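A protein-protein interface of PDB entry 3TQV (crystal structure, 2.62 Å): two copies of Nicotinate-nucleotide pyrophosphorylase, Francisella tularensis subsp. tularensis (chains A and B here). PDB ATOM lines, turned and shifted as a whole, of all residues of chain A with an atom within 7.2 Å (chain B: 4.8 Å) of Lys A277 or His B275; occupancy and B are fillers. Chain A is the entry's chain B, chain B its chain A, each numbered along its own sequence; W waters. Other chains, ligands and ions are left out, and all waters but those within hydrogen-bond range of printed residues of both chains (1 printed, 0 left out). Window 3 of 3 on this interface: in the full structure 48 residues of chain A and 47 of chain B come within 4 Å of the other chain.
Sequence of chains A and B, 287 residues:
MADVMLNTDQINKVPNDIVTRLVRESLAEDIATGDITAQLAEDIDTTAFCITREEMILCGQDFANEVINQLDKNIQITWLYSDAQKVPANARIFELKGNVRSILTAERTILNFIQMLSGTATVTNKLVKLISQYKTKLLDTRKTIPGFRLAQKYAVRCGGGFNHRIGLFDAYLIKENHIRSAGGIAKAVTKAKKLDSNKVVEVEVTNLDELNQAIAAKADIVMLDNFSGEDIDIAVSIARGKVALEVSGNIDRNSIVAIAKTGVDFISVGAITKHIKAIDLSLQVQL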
ATOM      1  N   GLU A  54     -10.843 -26.838   8.333  1.00  0.00           N
ATOM      2  CA  GLU A  54      -9.394 -26.688   8.328  1.00  0.00           C
ATOM      3  C   GLU A  54      -8.996 -25.291   8.737  1.00  0.00           C
ATOM      4  O   GLU A  54      -9.781 -24.370   8.634  1.00  0.00           O
ATOM      5  CB  GLU A  54      -8.832 -27.019   6.947  1.00  0.00           C
ATOM      6  CG  GLU A  54      -9.619 -26.383   5.809  1.00  0.00           C
ATOM      7  CD  GLU A  54      -8.958 -26.550   4.452  1.00  0.00           C
ATOM      8  OE1 GLU A  54      -9.665 -26.990   3.507  1.00  0.00           O
ATOM      9  OE2 GLU A  54      -7.744 -26.230   4.332  1.00  0.00           O
ATOM     10  N   GLN A 115     -14.963 -19.633   0.518  1.00  0.00           N
ATOM     11  CA  GLN A 115     -14.033 -20.671   0.055  1.00  0.00           C
ATOM     12  C   GLN A 115     -12.879 -20.069  -0.692  1.00  0.00           C
ATOM     13  O   GLN A 115     -11.717 -20.408  -0.480  1.00  0.00           O
ATOM     14  CB  GLN A 115     -14.711 -21.553  -0.975  1.00  0.00           C
ATOM     15  CG  GLN A 115     -15.521 -22.668  -0.449  1.00  0.00           C
ATOM     16  CD  GLN A 115     -16.257 -23.343  -1.565  1.00  0.00           C
ATOM     17  OE1 GLN A 115     -16.105 -22.982  -2.740  1.00  0.00           O
ATOM     18  NE2 GLN A 115     -17.068 -24.324  -1.215  1.00  0.00           N
ATOM     19  N   MET A 116     -13.247 -19.201  -1.618  1.00  0.00           N
ATOM     20  CA  MET A 116     -12.332 -18.684  -2.594  1.00  0.00           C
ATOM     21  C   MET A 116     -11.397 -17.671  -1.961  1.00  0.00           C
ATOM     22  O   MET A 116     -10.176 -17.853  -1.953  1.00  0.00           O
ATOM     23  CB  MET A 116     -13.124 -18.037  -3.716  1.00  0.00           C
ATOM     24  CG  MET A 116     -12.276 -17.639  -4.887  1.00  0.00           C
ATOM     25  SD  MET A 116     -13.169 -16.275  -5.912  1.00  0.00           S
ATOM     26  CE  MET A 116     -11.636 -15.670  -6.949  1.00  0.00           C
ATOM     27  N   SER A 118     -10.984 -16.778   1.175  1.00  0.00           N
ATOM     28  CA  SER A 118     -10.250 -17.273   2.326  1.00  0.00           C
ATOM     29  C   SER A 118      -9.144 -18.155   1.794  1.00  0.00           C
ATOM     30  O   SER A 118      -8.069 -18.258   2.386  1.00  0.00           O
ATOM     31  CB  SER A 118     -11.156 -18.074   3.255  1.00  0.00           C
ATOM     32  OG  SER A 118     -12.233 -17.291   3.716  1.00  0.00           O
ATOM     33  N   GLY A 119      -9.412 -18.797   0.666  1.00  0.00           N
ATOM     34  CA  GLY A 119      -8.398 -19.593   0.013  1.00  0.00           C
ATOM     35  C   GLY A 119      -7.211 -18.706  -0.306  1.00  0.00           C
ATOM     36  O   GLY A 119      -6.088 -18.940   0.164  1.00  0.00           O
ATOM     37  N   THR A 120      -7.471 -17.677  -1.105  1.00  0.00           N
ATOM     38  CA  THR A 120      -6.452 -16.712  -1.445  1.00  0.00           C
ATOM     39  C   THR A 120      -5.737 -16.153  -0.226  1.00  0.00           C
ATOM     40  O   THR A 120      -4.511 -16.065  -0.224  1.00  0.00           O
ATOM     41  CB  THR A 120      -7.000 -15.576  -2.304  1.00  0.00           C
ATOM     42  OG1 THR A 120      -7.312 -16.088  -3.602  1.00  0.00           O
ATOM     43  CG2 THR A 120      -5.952 -14.453  -2.454  1.00  0.00           C
ATOM     44  N   THR A 122      -5.418 -17.436   2.800  1.00  0.00           N
ATOM     45  CA  THR A 122      -4.668 -18.525   3.428  1.00  0.00           C
ATOM     46  C   THR A 122      -3.368 -18.901   2.683  1.00  0.00           C
ATOM     47  O   THR A 122      -2.350 -19.211   3.315  1.00  0.00           O
ATOM     48  CB  THR A 122      -5.584 -19.762   3.606  1.00  0.00           C
ATOM     49  OG1 THR A 122      -6.769 -19.366   4.318  1.00  0.00           O
ATOM     50  CG2 THR A 122      -4.873 -20.908   4.341  1.00  0.00           C
ATOM     51  N   VAL A 123      -3.386 -18.866   1.354  1.00  0.00           N
ATOM     52  CA  VAL A 123      -2.152 -19.079   0.596  1.00  0.00           C
ATOM     53  C   VAL A 123      -1.128 -18.021   0.985  1.00  0.00           C
ATOM     54  O   VAL A 123       0.045 -18.303   1.222  1.00  0.00           O
ATOM     55  CB  VAL A 123      -2.357 -18.883  -0.919  1.00  0.00           C
ATOM     56  CG1 VAL A 123      -1.119 -19.343  -1.660  1.00  0.00           C
ATOM     57  CG2 VAL A 123      -3.585 -19.605  -1.386  1.00  0.00           C
ATOM     58  N   LYS A 126       0.413 -18.434   4.440  1.00  0.00           N
ATOM     59  CA  LYS A 126       1.471 -19.438   4.454  1.00  0.00           C
ATOM     60  C   LYS A 126       2.818 -18.821   4.066  1.00  0.00           C
ATOM     61  O   LYS A 126       3.745 -18.790   4.868  1.00  0.00           O
ATOM     62  CB  LYS A 126       1.135 -20.649   3.574  1.00  0.00           C
ATOM     63  CG  LYS A 126       0.474 -21.789   4.343  1.00  0.00           C
ATOM     64  CD  LYS A 126      -0.670 -22.420   3.543  1.00  0.00           C
ATOM     65  CE  LYS A 126      -1.579 -23.291   4.412  1.00  0.00           C
ATOM     66  NZ  LYS A 126      -2.837 -23.659   3.676  1.00  0.00           N
ATOM     67  N   HIS A 275      -3.528 -19.344  -8.739  1.00  0.00           N
ATOM     68  CA  HIS A 275      -4.123 -20.613  -8.353  1.00  0.00           C
ATOM     69  C   HIS A 275      -5.117 -20.362  -7.232  1.00  0.00           C
ATOM     70  O   HIS A 275      -5.087 -19.308  -6.604  1.00  0.00           O
ATOM     71  CB  HIS A 275      -3.042 -21.588  -7.879  1.00  0.00           C
ATOM     72  CG  HIS A 275      -1.915 -21.762  -8.848  1.00  0.00           C
ATOM     73  ND1 HIS A 275      -2.096 -21.726 -10.214  1.00  0.00           N
ATOM     74  CD2 HIS A 275      -0.591 -21.961  -8.651  1.00  0.00           C
ATOM     75  CE1 HIS A 275      -0.933 -21.909 -10.818  1.00  0.00           C
ATOM     76  NE2 HIS A 275      -0.004 -22.051  -9.891  1.00  0.00           N
ATOM     77  N   ILE A 276      -6.003 -21.324  -6.996  1.00  0.00           N
ATOM     78  CA  ILE A 276      -6.890 -21.287  -5.838  1.00  0.00           C
ATOM     79  C   ILE A 276      -6.913 -22.625  -5.112  1.00  0.00           C
ATOM     80  O   ILE A 276      -7.218 -23.657  -5.701  1.00  0.00           O
ATOM     81  CB  ILE A 276      -8.335 -20.957  -6.212  1.00  0.00           C
ATOM     82  CG1 ILE A 276      -8.417 -19.681  -7.065  1.00  0.00           C
ATOM     83  CG2 ILE A 276      -9.144 -20.785  -4.962  1.00  0.00           C
ATOM     84  CD1 ILE A 276      -8.150 -18.377  -6.300  1.00  0.00           C
ATOM     85  N   LYS A 277      -6.582 -22.617  -3.828  1.00  0.00           N
ATOM     86  CA  LYS A 277      -6.861 -23.765  -2.981  1.00  0.00           C
ATOM     87  C   LYS A 277      -8.035 -23.352  -2.105  1.00  0.00           C
ATOM     88  O   LYS A 277      -7.867 -22.644  -1.112  1.00  0.00           O
ATOM     89  CB  LYS A 277      -5.635 -24.144  -2.148  1.00  0.00           C
ATOM     90  CG  LYS A 277      -5.787 -25.407  -1.320  1.00  0.00           C
ATOM     91  CD  LYS A 277      -6.174 -26.618  -2.181  1.00  0.00           C
ATOM     92  CE  LYS A 277      -6.790 -27.768  -1.347  1.00  0.00           C
ATOM     93  NZ  LYS A 277      -5.829 -28.435  -0.412  1.00  0.00           N
ATOM     94  N   ALA A 278      -9.238 -23.748  -2.499  1.00  0.00           N
ATOM     95  CA  ALA A 278     -10.423 -23.392  -1.721  1.00  0.00           C
ATOM     96  C   ALA A 278     -10.425 -24.038  -0.329  1.00  0.00           C
ATOM     97  O   ALA A 278     -10.070 -25.209  -0.151  1.00  0.00           O
ATOM     98  CB  ALA A 278     -11.703 -23.734  -2.476  1.00  0.00           C
ATOM     99  N   ILE A 279     -10.809 -23.240   0.656  1.00  0.00           N
ATOM    100  CA  ILE A 279     -11.001 -23.727   2.003  1.00  0.00           C
ATOM    101  C   ILE A 279     -12.268 -24.557   2.077  1.00  0.00           C
ATOM    102  O   ILE A 279     -13.299 -24.188   1.507  1.00  0.00           O
ATOM    103  CB  ILE A 279     -11.133 -22.560   3.000  1.00  0.00           C
ATOM    104  CG1 ILE A 279      -9.836 -21.735   3.022  1.00  0.00           C
ATOM    105  CG2 ILE A 279     -11.516 -23.081   4.375  1.00  0.00           C
ATOM    106  CD1 ILE A 279      -8.539 -22.575   2.932  1.00  0.00           C
ATOM    107  N   ASP A 280     -12.186 -25.673   2.794  1.00  0.00           N
ATOM    108  CA  ASP A 280     -13.330 -26.549   2.977  1.00  0.00           C
ATOM    109  C   ASP A 280     -14.277 -26.051   4.079  1.00  0.00           C
ATOM    110  O   ASP A 280     -13.908 -25.910   5.270  1.00  0.00           O
ATOM    111  CB  ASP A 280     -12.861 -27.977   3.251  1.00  0.00           C
ATOM    112  CG  ASP A 280     -13.994 -28.959   3.308  1.00  0.00           C
ATOM    113  OD1 ASP A 280     -15.063 -28.691   2.720  1.00  0.00           O
ATOM    114  OD2 ASP A 280     -13.811 -30.010   3.944  1.00  0.00           O
ATOM    115  N   GLY B 270     -16.132 -31.744  -6.710  1.00  0.00           N
ATOM    116  CA  GLY B 270     -16.147 -30.299  -6.620  1.00  0.00           C
ATOM    117  C   GLY B 270     -14.763 -29.727  -6.834  1.00  0.00           C
ATOM    118  O   GLY B 270     -14.611 -28.557  -7.200  1.00  0.00           O
ATOM    119  N   ALA B 271     -13.757 -30.566  -6.602  1.00  0.00           N
ATOM    120  CA  ALA B 271     -12.352 -30.174  -6.724  1.00  0.00           C
ATOM    121  C   ALA B 271     -12.028 -29.656  -8.111  1.00  0.00           C
ATOM    122  O   ALA B 271     -11.152 -28.819  -8.282  1.00  0.00           O
ATOM    123  CB  ALA B 271     -11.427 -31.350  -6.372  1.00  0.00           C
ATOM    124  N   ILE B 272     -12.731 -30.152  -9.115  1.00  0.00           N
ATOM    125  CA  ILE B 272     -12.374 -29.768 -10.469  1.00  0.00           C
ATOM    126  C   ILE B 272     -12.675 -28.298 -10.769  1.00  0.00           C
ATOM    127  O   ILE B 272     -12.033 -27.713 -11.648  1.00  0.00           O
ATOM    128  CB  ILE B 272     -12.952 -30.721 -11.523  1.00  0.00           C
ATOM    129  CG1 ILE B 272     -14.476 -30.722 -11.493  1.00  0.00           C
ATOM    130  CG2 ILE B 272     -12.407 -32.130 -11.307  1.00  0.00           C
ATOM    131  CD1 ILE B 272     -15.104 -31.474 -12.665  1.00  0.00           C
ATOM    132  N   THR B 273     -13.599 -27.698 -10.011  1.00  0.00           N
ATOM    133  CA  THR B 273     -13.957 -26.287 -10.192  1.00  0.00           C
ATOM    134  C   THR B 273     -13.713 -25.356  -8.988  1.00  0.00           C
ATOM    135  O   THR B 273     -13.448 -24.171  -9.178  1.00  0.00           O
ATOM    136  CB  THR B 273     -15.409 -26.113 -10.658  1.00  0.00           C
ATOM    137  OG1 THR B 273     -16.299 -26.701  -9.699  1.00  0.00           O
ATOM    138  CG2 THR B 273     -15.616 -26.768 -12.005  1.00  0.00           C
ATOM    139  N   LYS B 274     -13.810 -25.862  -7.760  1.00  0.00           N
ATOM    140  CA  LYS B 274     -13.562 -25.010  -6.587  1.00  0.00           C
ATOM    141  C   LYS B 274     -12.084 -24.677  -6.398  1.00  0.00           C
ATOM    142  O   LYS B 274     -11.732 -23.674  -5.771  1.00  0.00           O
ATOM    143  CB  LYS B 274     -14.097 -25.649  -5.309  1.00  0.00           C
ATOM    144  CG  LYS B 274     -13.279 -26.826  -4.787  1.00  0.00           C
ATOM    145  CD  LYS B 274     -14.032 -27.499  -3.665  1.00  0.00           C
ATOM    146  CE  LYS B 274     -13.295 -28.699  -3.128  1.00  0.00           C
ATOM    147  NZ  LYS B 274     -14.121 -29.391  -2.089  1.00  0.00           N
ATOM    148  N   HIS B 275     -11.214 -25.530  -6.922  1.00  0.00           N
ATOM    149  CA  HIS B 275      -9.797 -25.227  -6.913  1.00  0.00           C
ATOM    150  C   HIS B 275      -9.412 -24.744  -8.301  1.00  0.00           C
ATOM    151  O   HIS B 275     -10.138 -24.970  -9.267  1.00  0.00           O
ATOM    152  CB  HIS B 275      -8.974 -26.443  -6.474  1.00  0.00           C
ATOM    153  CG  HIS B 275      -9.300 -26.919  -5.089  1.00  0.00           C
ATOM    154  ND1 HIS B 275      -8.948 -28.167  -4.624  1.00  0.00           N
ATOM    155  CD2 HIS B 275      -9.961 -26.313  -4.072  1.00  0.00           C
ATOM    156  CE1 HIS B 275      -9.374 -28.311  -3.380  1.00  0.00           C
ATOM    157  NE2 HIS B 275      -9.994 -27.201  -3.023  1.00  0.00           N
ATOM    158  N   ILE B 276      -8.297 -24.034  -8.398  1.00  0.00           N
ATOM    159  CA  ILE B 276      -7.825 -23.562  -9.686  1.00  0.00           C
ATOM    160  C   ILE B 276      -6.331 -23.789  -9.739  1.00  0.00           C
ATOM    161  O   ILE B 276      -5.588 -23.267  -8.912  1.00  0.00           O
ATOM    162  CB  ILE B 276      -8.124 -22.048  -9.912  1.00  0.00           C
ATOM    163  CG1 ILE B 276      -9.637 -21.734  -9.795  1.00  0.00           C
ATOM    164  CG2 ILE B 276      -7.535 -21.564 -11.251  1.00  0.00           C
ATOM    165  CD1 ILE B 276     -10.501 -22.279 -10.920  1.00  0.00           C
ATOM    166  N   LYS B 277      -5.894 -24.592 -10.702  1.00  0.00           N
ATOM    167  CA  LYS B 277      -4.481 -24.730 -10.999  1.00  0.00           C
ATOM    168  C   LYS B 277      -4.237 -24.079 -12.344  1.00  0.00           C
ATOM    169  O   LYS B 277      -4.512 -24.685 -13.377  1.00  0.00           O
ATOM    170  CB  LYS B 277      -4.101 -26.201 -11.067  1.00  0.00           C
ATOM    171  CG  LYS B 277      -2.602 -26.454 -11.137  1.00  0.00           C
ATOM    172  CD  LYS B 277      -1.931 -26.138  -9.812  1.00  0.00           C
ATOM    173  CE  LYS B 277      -0.423 -26.273  -9.954  1.00  0.00           C
ATOM    174  NZ  LYS B 277      -0.099 -27.369 -10.917  1.00  0.00           N
HETATM  175  O   HOH W   1     -13.029 -21.446  -4.270  1.00  0.00           O
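Hydrophobic or aromatic side chains of chain A within 4 Å of the printed part of chain B: His A275, Ile A276 and Ala A278. Of the 8 printed residues of chain B, 4 touch a printed residue of chain A.
Among the printed residues, merely in contact across the chains: His A275 with Ile B276 (3.1 Å), Ile A276 with His B275 (3.3 Å), Ala A278 with Lys B274 (3.3 Å), Lys A277 with His B275 (3.3 Å), His A275 with Lys B277 (3.8 Å) and Ile A276 with Lys B274 (3.96 Å).
His A275 touches Ile B276, and with the chains exchanged Ile A276 touches His B275. His A275 touches Lys B277, and with the chains exchanged Lys A277 touches His B275. Ile B276 touches its own counterpart, Ile A276. Of the 8 pairs that touch across the chains among the printed residues, 5 have their exchanged pair printed and touching as well.
Gly A119 touches none of the printed residues of chain B. Lys A277 touches just one residue of chain B: His B275 (3.3 Å). Of the printed residues of chain B, Ala A278 touches Lys B274 and His B275. Gly B270 touches none of the printed residues of chain A. Of the printed residues of chain A, His B275 touches Ile A276 (3.3 Å), Lys A277 (3.3 Å) and Ala A278 (3.1 Å). Of the printed residues of chain A, Ile B276 touches His A275 (3.1 Å) and Ile A276 (2.8 Å). The nearest residue of chain A that does not touch His B275 is Ile A279 (5.5 Å). The nearest printed residue of chain B that does not touch Ile A276 is Lys B277 (4.9 Å).
The backbone carbonyl oxygen (O) of Ala A278 lies within hydrogen-bond range of a ring nitrogen (NE2) of His B275 (3.5 Å). N of Ile A276 lies within hydrogen-bond range of O of Ile B276, 2.8 Å away.
Water W1 lies within hydrogen-bond range of the backbone carbonyl oxygen of Lys B274 (3.0 Å) and the backbone NH of Met A116 (3.5 Å).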
